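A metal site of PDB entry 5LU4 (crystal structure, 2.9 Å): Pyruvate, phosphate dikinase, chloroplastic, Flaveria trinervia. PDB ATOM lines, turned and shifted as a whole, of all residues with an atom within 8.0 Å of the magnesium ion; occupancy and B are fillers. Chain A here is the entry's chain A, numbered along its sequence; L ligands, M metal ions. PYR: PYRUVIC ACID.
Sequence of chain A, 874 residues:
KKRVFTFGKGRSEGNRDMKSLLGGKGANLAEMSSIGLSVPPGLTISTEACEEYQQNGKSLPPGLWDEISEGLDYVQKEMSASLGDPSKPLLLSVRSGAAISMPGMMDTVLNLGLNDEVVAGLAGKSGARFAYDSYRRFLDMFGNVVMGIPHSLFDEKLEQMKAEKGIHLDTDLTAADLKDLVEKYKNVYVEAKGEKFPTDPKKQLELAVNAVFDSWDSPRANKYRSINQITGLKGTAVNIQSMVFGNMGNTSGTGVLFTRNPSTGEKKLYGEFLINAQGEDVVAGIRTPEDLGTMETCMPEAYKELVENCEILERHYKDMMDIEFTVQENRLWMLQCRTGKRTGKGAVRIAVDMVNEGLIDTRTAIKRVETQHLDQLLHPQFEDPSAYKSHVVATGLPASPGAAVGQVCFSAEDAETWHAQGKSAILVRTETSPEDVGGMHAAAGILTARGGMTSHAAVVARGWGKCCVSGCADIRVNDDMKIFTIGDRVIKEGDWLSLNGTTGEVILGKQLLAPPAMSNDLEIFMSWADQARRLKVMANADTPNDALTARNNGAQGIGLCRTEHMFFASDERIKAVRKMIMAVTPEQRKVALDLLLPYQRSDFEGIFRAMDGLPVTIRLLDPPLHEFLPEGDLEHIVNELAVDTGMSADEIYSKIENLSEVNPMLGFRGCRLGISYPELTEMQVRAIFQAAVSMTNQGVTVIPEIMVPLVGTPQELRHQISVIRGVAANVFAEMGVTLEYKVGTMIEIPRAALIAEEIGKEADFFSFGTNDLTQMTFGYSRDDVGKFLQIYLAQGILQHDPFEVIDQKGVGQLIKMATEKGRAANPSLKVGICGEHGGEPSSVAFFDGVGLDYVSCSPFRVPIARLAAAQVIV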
ATOM      1  N   LEU A 560     -27.491 -21.388  -2.081  1.00  0.00           N
ATOM      2  CA  LEU A 560     -26.392 -20.452  -1.991  1.00  0.00           C
ATOM      3  C   LEU A 560     -26.866 -19.049  -2.216  1.00  0.00           C
ATOM      4  O   LEU A 560     -27.410 -18.764  -3.264  1.00  0.00           O
ATOM      5  CB  LEU A 560     -25.332 -20.794  -3.025  1.00  0.00           C
ATOM      6  CG  LEU A 560     -24.026 -20.016  -2.903  1.00  0.00           C
ATOM      7  CD1 LEU A 560     -23.332 -20.425  -1.612  1.00  0.00           C
ATOM      8  CD2 LEU A 560     -23.141 -20.246  -4.113  1.00  0.00           C
ATOM      9  N   ARG A 562     -25.000 -15.480  -2.113  1.00  0.00           N
ATOM     10  CA  ARG A 562     -23.720 -14.820  -1.987  1.00  0.00           C
ATOM     11  C   ARG A 562     -23.915 -13.428  -1.424  1.00  0.00           C
ATOM     12  O   ARG A 562     -24.645 -12.624  -2.001  1.00  0.00           O
ATOM     13  CB  ARG A 562     -23.018 -14.771  -3.342  1.00  0.00           C
ATOM     14  CG  ARG A 562     -22.674 -16.148  -3.907  1.00  0.00           C
ATOM     15  CD  ARG A 562     -21.881 -16.088  -5.202  1.00  0.00           C
ATOM     16  NE  ARG A 562     -22.673 -15.552  -6.323  1.00  0.00           N
ATOM     17  CZ  ARG A 562     -22.532 -14.348  -6.892  1.00  0.00           C
ATOM     18  NH1 ARG A 562     -21.605 -13.470  -6.498  1.00  0.00           N
ATOM     19  NH2 ARG A 562     -23.333 -14.003  -7.883  1.00  0.00           N
ATOM     20  N   GLU A 564     -21.667 -11.053  -1.067  1.00  0.00           N
ATOM     21  CA  GLU A 564     -20.952 -10.068  -1.851  1.00  0.00           C
ATOM     22  C   GLU A 564     -21.807  -9.471  -2.969  1.00  0.00           C
ATOM     23  O   GLU A 564     -21.633  -8.315  -3.342  1.00  0.00           O
ATOM     24  CB  GLU A 564     -19.651 -10.658  -2.410  1.00  0.00           C
ATOM     25  CG  GLU A 564     -19.799 -11.912  -3.275  1.00  0.00           C
ATOM     26  CD  GLU A 564     -19.758 -13.206  -2.491  1.00  0.00           C
ATOM     27  OE1 GLU A 564     -19.866 -13.171  -1.258  1.00  0.00           O
ATOM     28  OE2 GLU A 564     -19.600 -14.278  -3.084  1.00  0.00           O
ATOM     29  N   ARG A 619     -24.328 -17.871   2.473  1.00  0.00           N
ATOM     30  CA  ARG A 619     -22.899 -18.018   2.755  1.00  0.00           C
ATOM     31  C   ARG A 619     -22.352 -16.748   3.336  1.00  0.00           C
ATOM     32  O   ARG A 619     -22.944 -15.748   3.185  1.00  0.00           O
ATOM     33  CB  ARG A 619     -22.124 -18.320   1.497  1.00  0.00           C
ATOM     34  CG  ARG A 619     -21.949 -17.099   0.590  1.00  0.00           C
ATOM     35  CD  ARG A 619     -21.344 -17.453  -0.752  1.00  0.00           C
ATOM     36  NE  ARG A 619     -20.113 -18.152  -0.628  1.00  0.00           N
ATOM     37  CZ  ARG A 619     -19.471 -18.643  -1.676  1.00  0.00           C
ATOM     38  NH1 ARG A 619     -19.922 -18.518  -2.921  1.00  0.00           N
ATOM     39  NH2 ARG A 619     -18.313 -19.278  -1.470  1.00  0.00           N
ATOM     40  N   ASP A 622     -17.272 -14.475   0.998  1.00  0.00           N
ATOM     41  CA  ASP A 622     -16.264 -15.347   0.360  1.00  0.00           C
ATOM     42  C   ASP A 622     -15.088 -14.567  -0.232  1.00  0.00           C
ATOM     43  O   ASP A 622     -13.971 -14.703   0.236  1.00  0.00           O
ATOM     44  CB  ASP A 622     -16.898 -16.232  -0.727  1.00  0.00           C
ATOM     45  CG  ASP A 622     -15.970 -17.280  -1.217  1.00  0.00           C
ATOM     46  OD1 ASP A 622     -14.862 -17.401  -0.663  1.00  0.00           O
ATOM     47  OD2 ASP A 622     -16.347 -17.996  -2.179  1.00  0.00           O
ATOM     48  N   PRO A 623     -15.335 -13.740  -1.245  1.00  0.00           N
ATOM     49  CA  PRO A 623     -14.243 -13.294  -2.088  1.00  0.00           C
ATOM     50  C   PRO A 623     -13.329 -12.339  -1.364  1.00  0.00           C
ATOM     51  O   PRO A 623     -13.744 -11.781  -0.343  1.00  0.00           O
ATOM     52  CB  PRO A 623     -14.954 -12.576  -3.226  1.00  0.00           C
ATOM     53  CG  PRO A 623     -16.160 -12.017  -2.590  1.00  0.00           C
ATOM     54  CD  PRO A 623     -16.563 -12.991  -1.514  1.00  0.00           C
ATOM     55  N   MET A 665      -7.194 -16.216  -5.660  1.00  0.00           N
ATOM     56  CA  MET A 665      -8.037 -17.387  -5.444  1.00  0.00           C
ATOM     57  C   MET A 665      -7.787 -18.077  -4.099  1.00  0.00           C
ATOM     58  O   MET A 665      -8.692 -18.675  -3.550  1.00  0.00           O
ATOM     59  CB  MET A 665      -7.848 -18.393  -6.565  1.00  0.00           C
ATOM     60  CG  MET A 665      -8.746 -19.602  -6.462  1.00  0.00           C
ATOM     61  SD  MET A 665      -8.382 -20.756  -7.823  1.00  0.00           S
ATOM     62  CE  MET A 665      -6.719 -21.300  -7.429  1.00  0.00           C
ATOM     63  N   ARG A 669      -9.213 -14.620   2.117  1.00  0.00           N
ATOM     64  CA  ARG A 669     -10.472 -14.917   1.456  1.00  0.00           C
ATOM     65  C   ARG A 669     -11.306 -15.833   2.314  1.00  0.00           C
ATOM     66  O   ARG A 669     -10.790 -16.611   3.096  1.00  0.00           O
ATOM     67  CB  ARG A 669     -10.188 -15.619   0.102  1.00  0.00           C
ATOM     68  CG  ARG A 669     -11.415 -15.864  -0.735  1.00  0.00           C
ATOM     69  CD  ARG A 669     -11.129 -16.569  -2.017  1.00  0.00           C
ATOM     70  NE  ARG A 669     -12.356 -16.743  -2.761  1.00  0.00           N
ATOM     71  CZ  ARG A 669     -12.447 -17.318  -3.948  1.00  0.00           C
ATOM     72  NH1 ARG A 669     -11.349 -17.814  -4.516  1.00  0.00           N
ATOM     73  NH2 ARG A 669     -13.638 -17.429  -4.570  1.00  0.00           N
ATOM     74  N   GLY A 670     -12.613 -15.699   2.174  1.00  0.00           N
ATOM     75  CA  GLY A 670     -13.548 -16.612   2.807  1.00  0.00           C
ATOM     76  C   GLY A 670     -13.543 -16.426   4.298  1.00  0.00           C
ATOM     77  O   GLY A 670     -13.558 -15.294   4.799  1.00  0.00           O
ATOM     78  N   PRO A 709     -17.417 -20.390   4.350  1.00  0.00           N
ATOM     79  CA  PRO A 709     -16.607 -20.834   3.220  1.00  0.00           C
ATOM     80  C   PRO A 709     -15.141 -21.107   3.516  1.00  0.00           C
ATOM     81  O   PRO A 709     -14.626 -20.640   4.524  1.00  0.00           O
ATOM     82  CB  PRO A 709     -16.721 -19.668   2.244  1.00  0.00           C
ATOM     83  CG  PRO A 709     -16.842 -18.486   3.129  1.00  0.00           C
ATOM     84  CD  PRO A 709     -17.627 -18.947   4.332  1.00  0.00           C
ATOM     85  N   LEU A 710     -14.498 -21.839   2.601  1.00  0.00           N
ATOM     86  CA  LEU A 710     -13.050 -22.130   2.646  1.00  0.00           C
ATOM     87  C   LEU A 710     -12.599 -22.751   3.932  1.00  0.00           C
ATOM     88  O   LEU A 710     -11.511 -22.427   4.444  1.00  0.00           O
ATOM     89  CB  LEU A 710     -12.228 -20.868   2.364  1.00  0.00           C
ATOM     90  CG  LEU A 710     -12.082 -20.514   0.905  1.00  0.00           C
ATOM     91  CD1 LEU A 710     -11.372 -19.195   0.805  1.00  0.00           C
ATOM     92  CD2 LEU A 710     -11.303 -21.532   0.119  1.00  0.00           C
ATOM     93  N   MET A 746     -18.939 -24.914   3.582  1.00  0.00           N
ATOM     94  CA  MET A 746     -18.814 -25.236   2.192  1.00  0.00           C
ATOM     95  C   MET A 746     -17.540 -26.058   2.072  1.00  0.00           C
ATOM     96  O   MET A 746     -16.501 -25.669   2.591  1.00  0.00           O
ATOM     97  CB  MET A 746     -18.783 -23.974   1.308  1.00  0.00           C
ATOM     98  CG  MET A 746     -18.977 -24.300  -0.129  1.00  0.00           C
ATOM     99  SD  MET A 746     -18.817 -22.905  -1.207  1.00  0.00           S
ATOM    100  CE  MET A 746     -20.342 -22.023  -0.987  1.00  0.00           C
ATOM    101  N   GLU A 748     -14.881 -26.723  -0.069  1.00  0.00           N
ATOM    102  CA  GLU A 748     -14.120 -26.262  -1.233  1.00  0.00           C
ATOM    103  C   GLU A 748     -12.664 -26.783  -1.254  1.00  0.00           C
ATOM    104  O   GLU A 748     -12.094 -26.981  -2.268  1.00  0.00           O
ATOM    105  CB  GLU A 748     -14.097 -24.728  -1.274  1.00  0.00           C
ATOM    106  CG  GLU A 748     -15.438 -24.062  -1.623  1.00  0.00           C
ATOM    107  CD  GLU A 748     -15.393 -22.545  -1.554  1.00  0.00           C
ATOM    108  OE1 GLU A 748     -14.558 -22.018  -0.824  1.00  0.00           O
ATOM    109  OE2 GLU A 748     -16.186 -21.847  -2.225  1.00  0.00           O
ATOM    110  N   GLY A 769     -18.451 -26.834  -2.878  1.00  0.00           N
ATOM    111  CA  GLY A 769     -18.143 -25.805  -3.856  1.00  0.00           C
ATOM    112  C   GLY A 769     -17.193 -26.370  -4.918  1.00  0.00           C
ATOM    113  O   GLY A 769     -15.970 -26.257  -4.787  1.00  0.00           O
ATOM    114  N   THR A 770     -17.744 -26.967  -5.960  1.00  0.00           N
ATOM    115  CA  THR A 770     -16.953 -27.705  -6.909  1.00  0.00           C
ATOM    116  C   THR A 770     -16.186 -26.842  -7.906  1.00  0.00           C
ATOM    117  O   THR A 770     -15.353 -27.348  -8.628  1.00  0.00           O
ATOM    118  CB  THR A 770     -17.844 -28.682  -7.667  1.00  0.00           C
ATOM    119  OG1 THR A 770     -18.985 -27.975  -8.165  1.00  0.00           O
ATOM    120  CG2 THR A 770     -18.294 -29.774  -6.742  1.00  0.00           C
ATOM    121  N   ASN A 771     -16.464 -25.553  -7.945  1.00  0.00           N
ATOM    122  CA  ASN A 771     -15.599 -24.621  -8.645  1.00  0.00           C
ATOM    123  C   ASN A 771     -14.220 -24.589  -7.971  1.00  0.00           C
ATOM    124  O   ASN A 771     -13.215 -24.937  -8.582  1.00  0.00           O
ATOM    125  CB  ASN A 771     -16.226 -23.208  -8.714  1.00  0.00           C
ATOM    126  CG  ASN A 771     -17.470 -23.147  -9.579  1.00  0.00           C
ATOM    127  OD1 ASN A 771     -17.529 -23.780 -10.630  1.00  0.00           O
ATOM    128  ND2 ASN A 771     -18.446 -22.383  -9.157  1.00  0.00           N
ATOM    129  N   ASP A 772     -14.187 -24.157  -6.729  1.00  0.00           N
ATOM    130  CA  ASP A 772     -12.938 -24.070  -6.006  1.00  0.00           C
ATOM    131  C   ASP A 772     -12.322 -25.462  -5.778  1.00  0.00           C
ATOM    132  O   ASP A 772     -11.087 -25.610  -5.745  1.00  0.00           O
ATOM    133  CB  ASP A 772     -13.165 -23.346  -4.669  1.00  0.00           C
ATOM    134  CG  ASP A 772     -13.449 -21.860  -4.853  1.00  0.00           C
ATOM    135  OD1 ASP A 772     -12.991 -21.274  -5.896  1.00  0.00           O
ATOM    136  OD2 ASP A 772     -14.108 -21.262  -3.948  1.00  0.00           O
ATOM    137  N   LEU A 773     -13.159 -26.488  -5.631  1.00  0.00           N
ATOM    138  CA  LEU A 773     -12.628 -27.828  -5.383  1.00  0.00           C
ATOM    139  C   LEU A 773     -11.983 -28.407  -6.620  1.00  0.00           C
ATOM    140  O   LEU A 773     -10.955 -29.075  -6.540  1.00  0.00           O
ATOM    141  CB  LEU A 773     -13.730 -28.748  -4.858  1.00  0.00           C
ATOM    142  CG  LEU A 773     -13.341 -30.167  -4.526  1.00  0.00           C
ATOM    143  CD1 LEU A 773     -12.248 -30.241  -3.464  1.00  0.00           C
ATOM    144  CD2 LEU A 773     -14.593 -30.884  -4.056  1.00  0.00           C
ATOM    145  N   GLN A 775     -10.679 -26.475  -8.956  1.00  0.00           N
ATOM    146  CA  GLN A 775      -9.507 -25.639  -9.146  1.00  0.00           C
ATOM    147  C   GLN A 775      -8.307 -26.165  -8.338  1.00  0.00           C
ATOM    148  O   GLN A 775      -7.204 -26.319  -8.847  1.00  0.00           O
ATOM    149  CB  GLN A 775      -9.815 -24.174  -8.803  1.00  0.00           C
ATOM    150  CG  GLN A 775     -10.610 -23.417  -9.872  1.00  0.00           C
ATOM    151  CD  GLN A 775     -11.045 -22.014  -9.470  1.00  0.00           C
ATOM    152  OE1 GLN A 775     -11.092 -21.652  -8.308  1.00  0.00           O
ATOM    153  NE2 GLN A 775     -11.398 -21.229 -10.455  1.00  0.00           N
ATOM    154  N   MET A 776      -8.552 -26.474  -7.078  1.00  0.00           N
ATOM    155  CA  MET A 776      -7.471 -26.866  -6.196  1.00  0.00           C
ATOM    156  C   MET A 776      -7.100 -28.338  -6.313  1.00  0.00           C
ATOM    157  O   MET A 776      -6.017 -28.697  -5.946  1.00  0.00           O
ATOM    158  CB  MET A 776      -7.837 -26.521  -4.764  1.00  0.00           C
ATOM    159  CG  MET A 776      -7.829 -25.037  -4.532  1.00  0.00           C
ATOM    160  SD  MET A 776      -8.250 -24.724  -2.818  1.00  0.00           S
ATOM    161  CE  MET A 776     -10.049 -24.722  -2.794  1.00  0.00           C
ATOM    162  N   CYS A 834     -23.532 -26.518  -4.453  1.00  0.00           N
ATOM    163  CA  CYS A 834     -23.952 -25.251  -5.022  1.00  0.00           C
ATOM    164  C   CYS A 834     -22.939 -24.741  -6.045  1.00  0.00           C
ATOM    165  O   CYS A 834     -22.823 -23.519  -6.263  1.00  0.00           O
ATOM    166  CB  CYS A 834     -24.133 -24.198  -3.916  1.00  0.00           C
ATOM    167  SG  CYS A 834     -22.556 -23.850  -3.096  1.00  0.00           S
HETATM  168  C   PYR L   1     -17.526 -22.411  -5.422  1.00  0.00           C
HETATM  169  O   PYR L   1     -17.976 -23.427  -6.046  1.00  0.00           O
HETATM  170  OXT PYR L   1     -16.473 -22.464  -4.725  1.00  0.00           O
HETATM  171  CA  PYR L   1     -18.261 -21.147  -5.511  1.00  0.00           C
HETATM  172  O3  PYR L   1     -17.731 -20.117  -6.005  1.00  0.00           O
HETATM  173  CB  PYR L   1     -19.680 -21.201  -4.998  1.00  0.00           C
HETATM  174 MG    MG M   1     -15.750 -20.092  -3.471  1.00  0.00          MG
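The backbone NH (N) of Asp 772 lies close to an oxygen (OXT) of the ligand (3.5 Å).
The side-chain carboxylate (OD2) of Asp 772 lies close to an oxygen (OXT) of the ligand (2.8 Å).
An oxygen (OXT) of the ligand lies close to the side-chain carboxylate (OE2) of Glu 748 (2.6 Å).
The backbone NH of Asn 771 sits close to an oxygen (O) of the ligand, 3.2 Å away.
An oxygen (O) of the ligand lies close to the side-chain amide nitrogen (ND2) of Asn 771, 3.3 Å away.
The side-chain carboxylate of Asp 772 sits close to the guanidinium group of Arg 669 (3.9 Å).
OE1 of Gln 775 sits close to OD1 of Asp 772 (3.1 Å).
NH2 of Arg 619 sits close to OE2 of Glu 748, at 3.4 Å.
N of Leu 710 sits close to OE1 of Glu 748 (3.4 Å).
The side-chain carboxylate of Asp 622 lies within salt-bridge range of the guanidinium group of Arg 669.
O of Asp 622 sits at hydrogen-bond distance from N of Gly 670.
NH2 of Arg 619 sits close to SD of Met 746 (3.7 Å).
NH1 of Arg 669 is in hydrogen-bond range of O of Met 665, at 3.0 Å.
Arg 619 touches the magnesium ion.
NH2 of Arg 669 touches the magnesium ion, 3.6 Å away.
Within 4 Å of the magnesium ion: Arg 619, Asp 622, Arg 669, Glu 748 and Asp 772.
The magnesium ion is bound by the side-chain carboxylate of Asp 772 (2.1 Å), the side-chain carboxylate of Glu 748 (2.2 Å) and the side-chain carboxylate of Asp 622 (2.5 Å).
The magnesium ion has three donor atoms within binding distance.
Slightly farther from the magnesium ion lies OXT of the ligand (2.8 Å).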
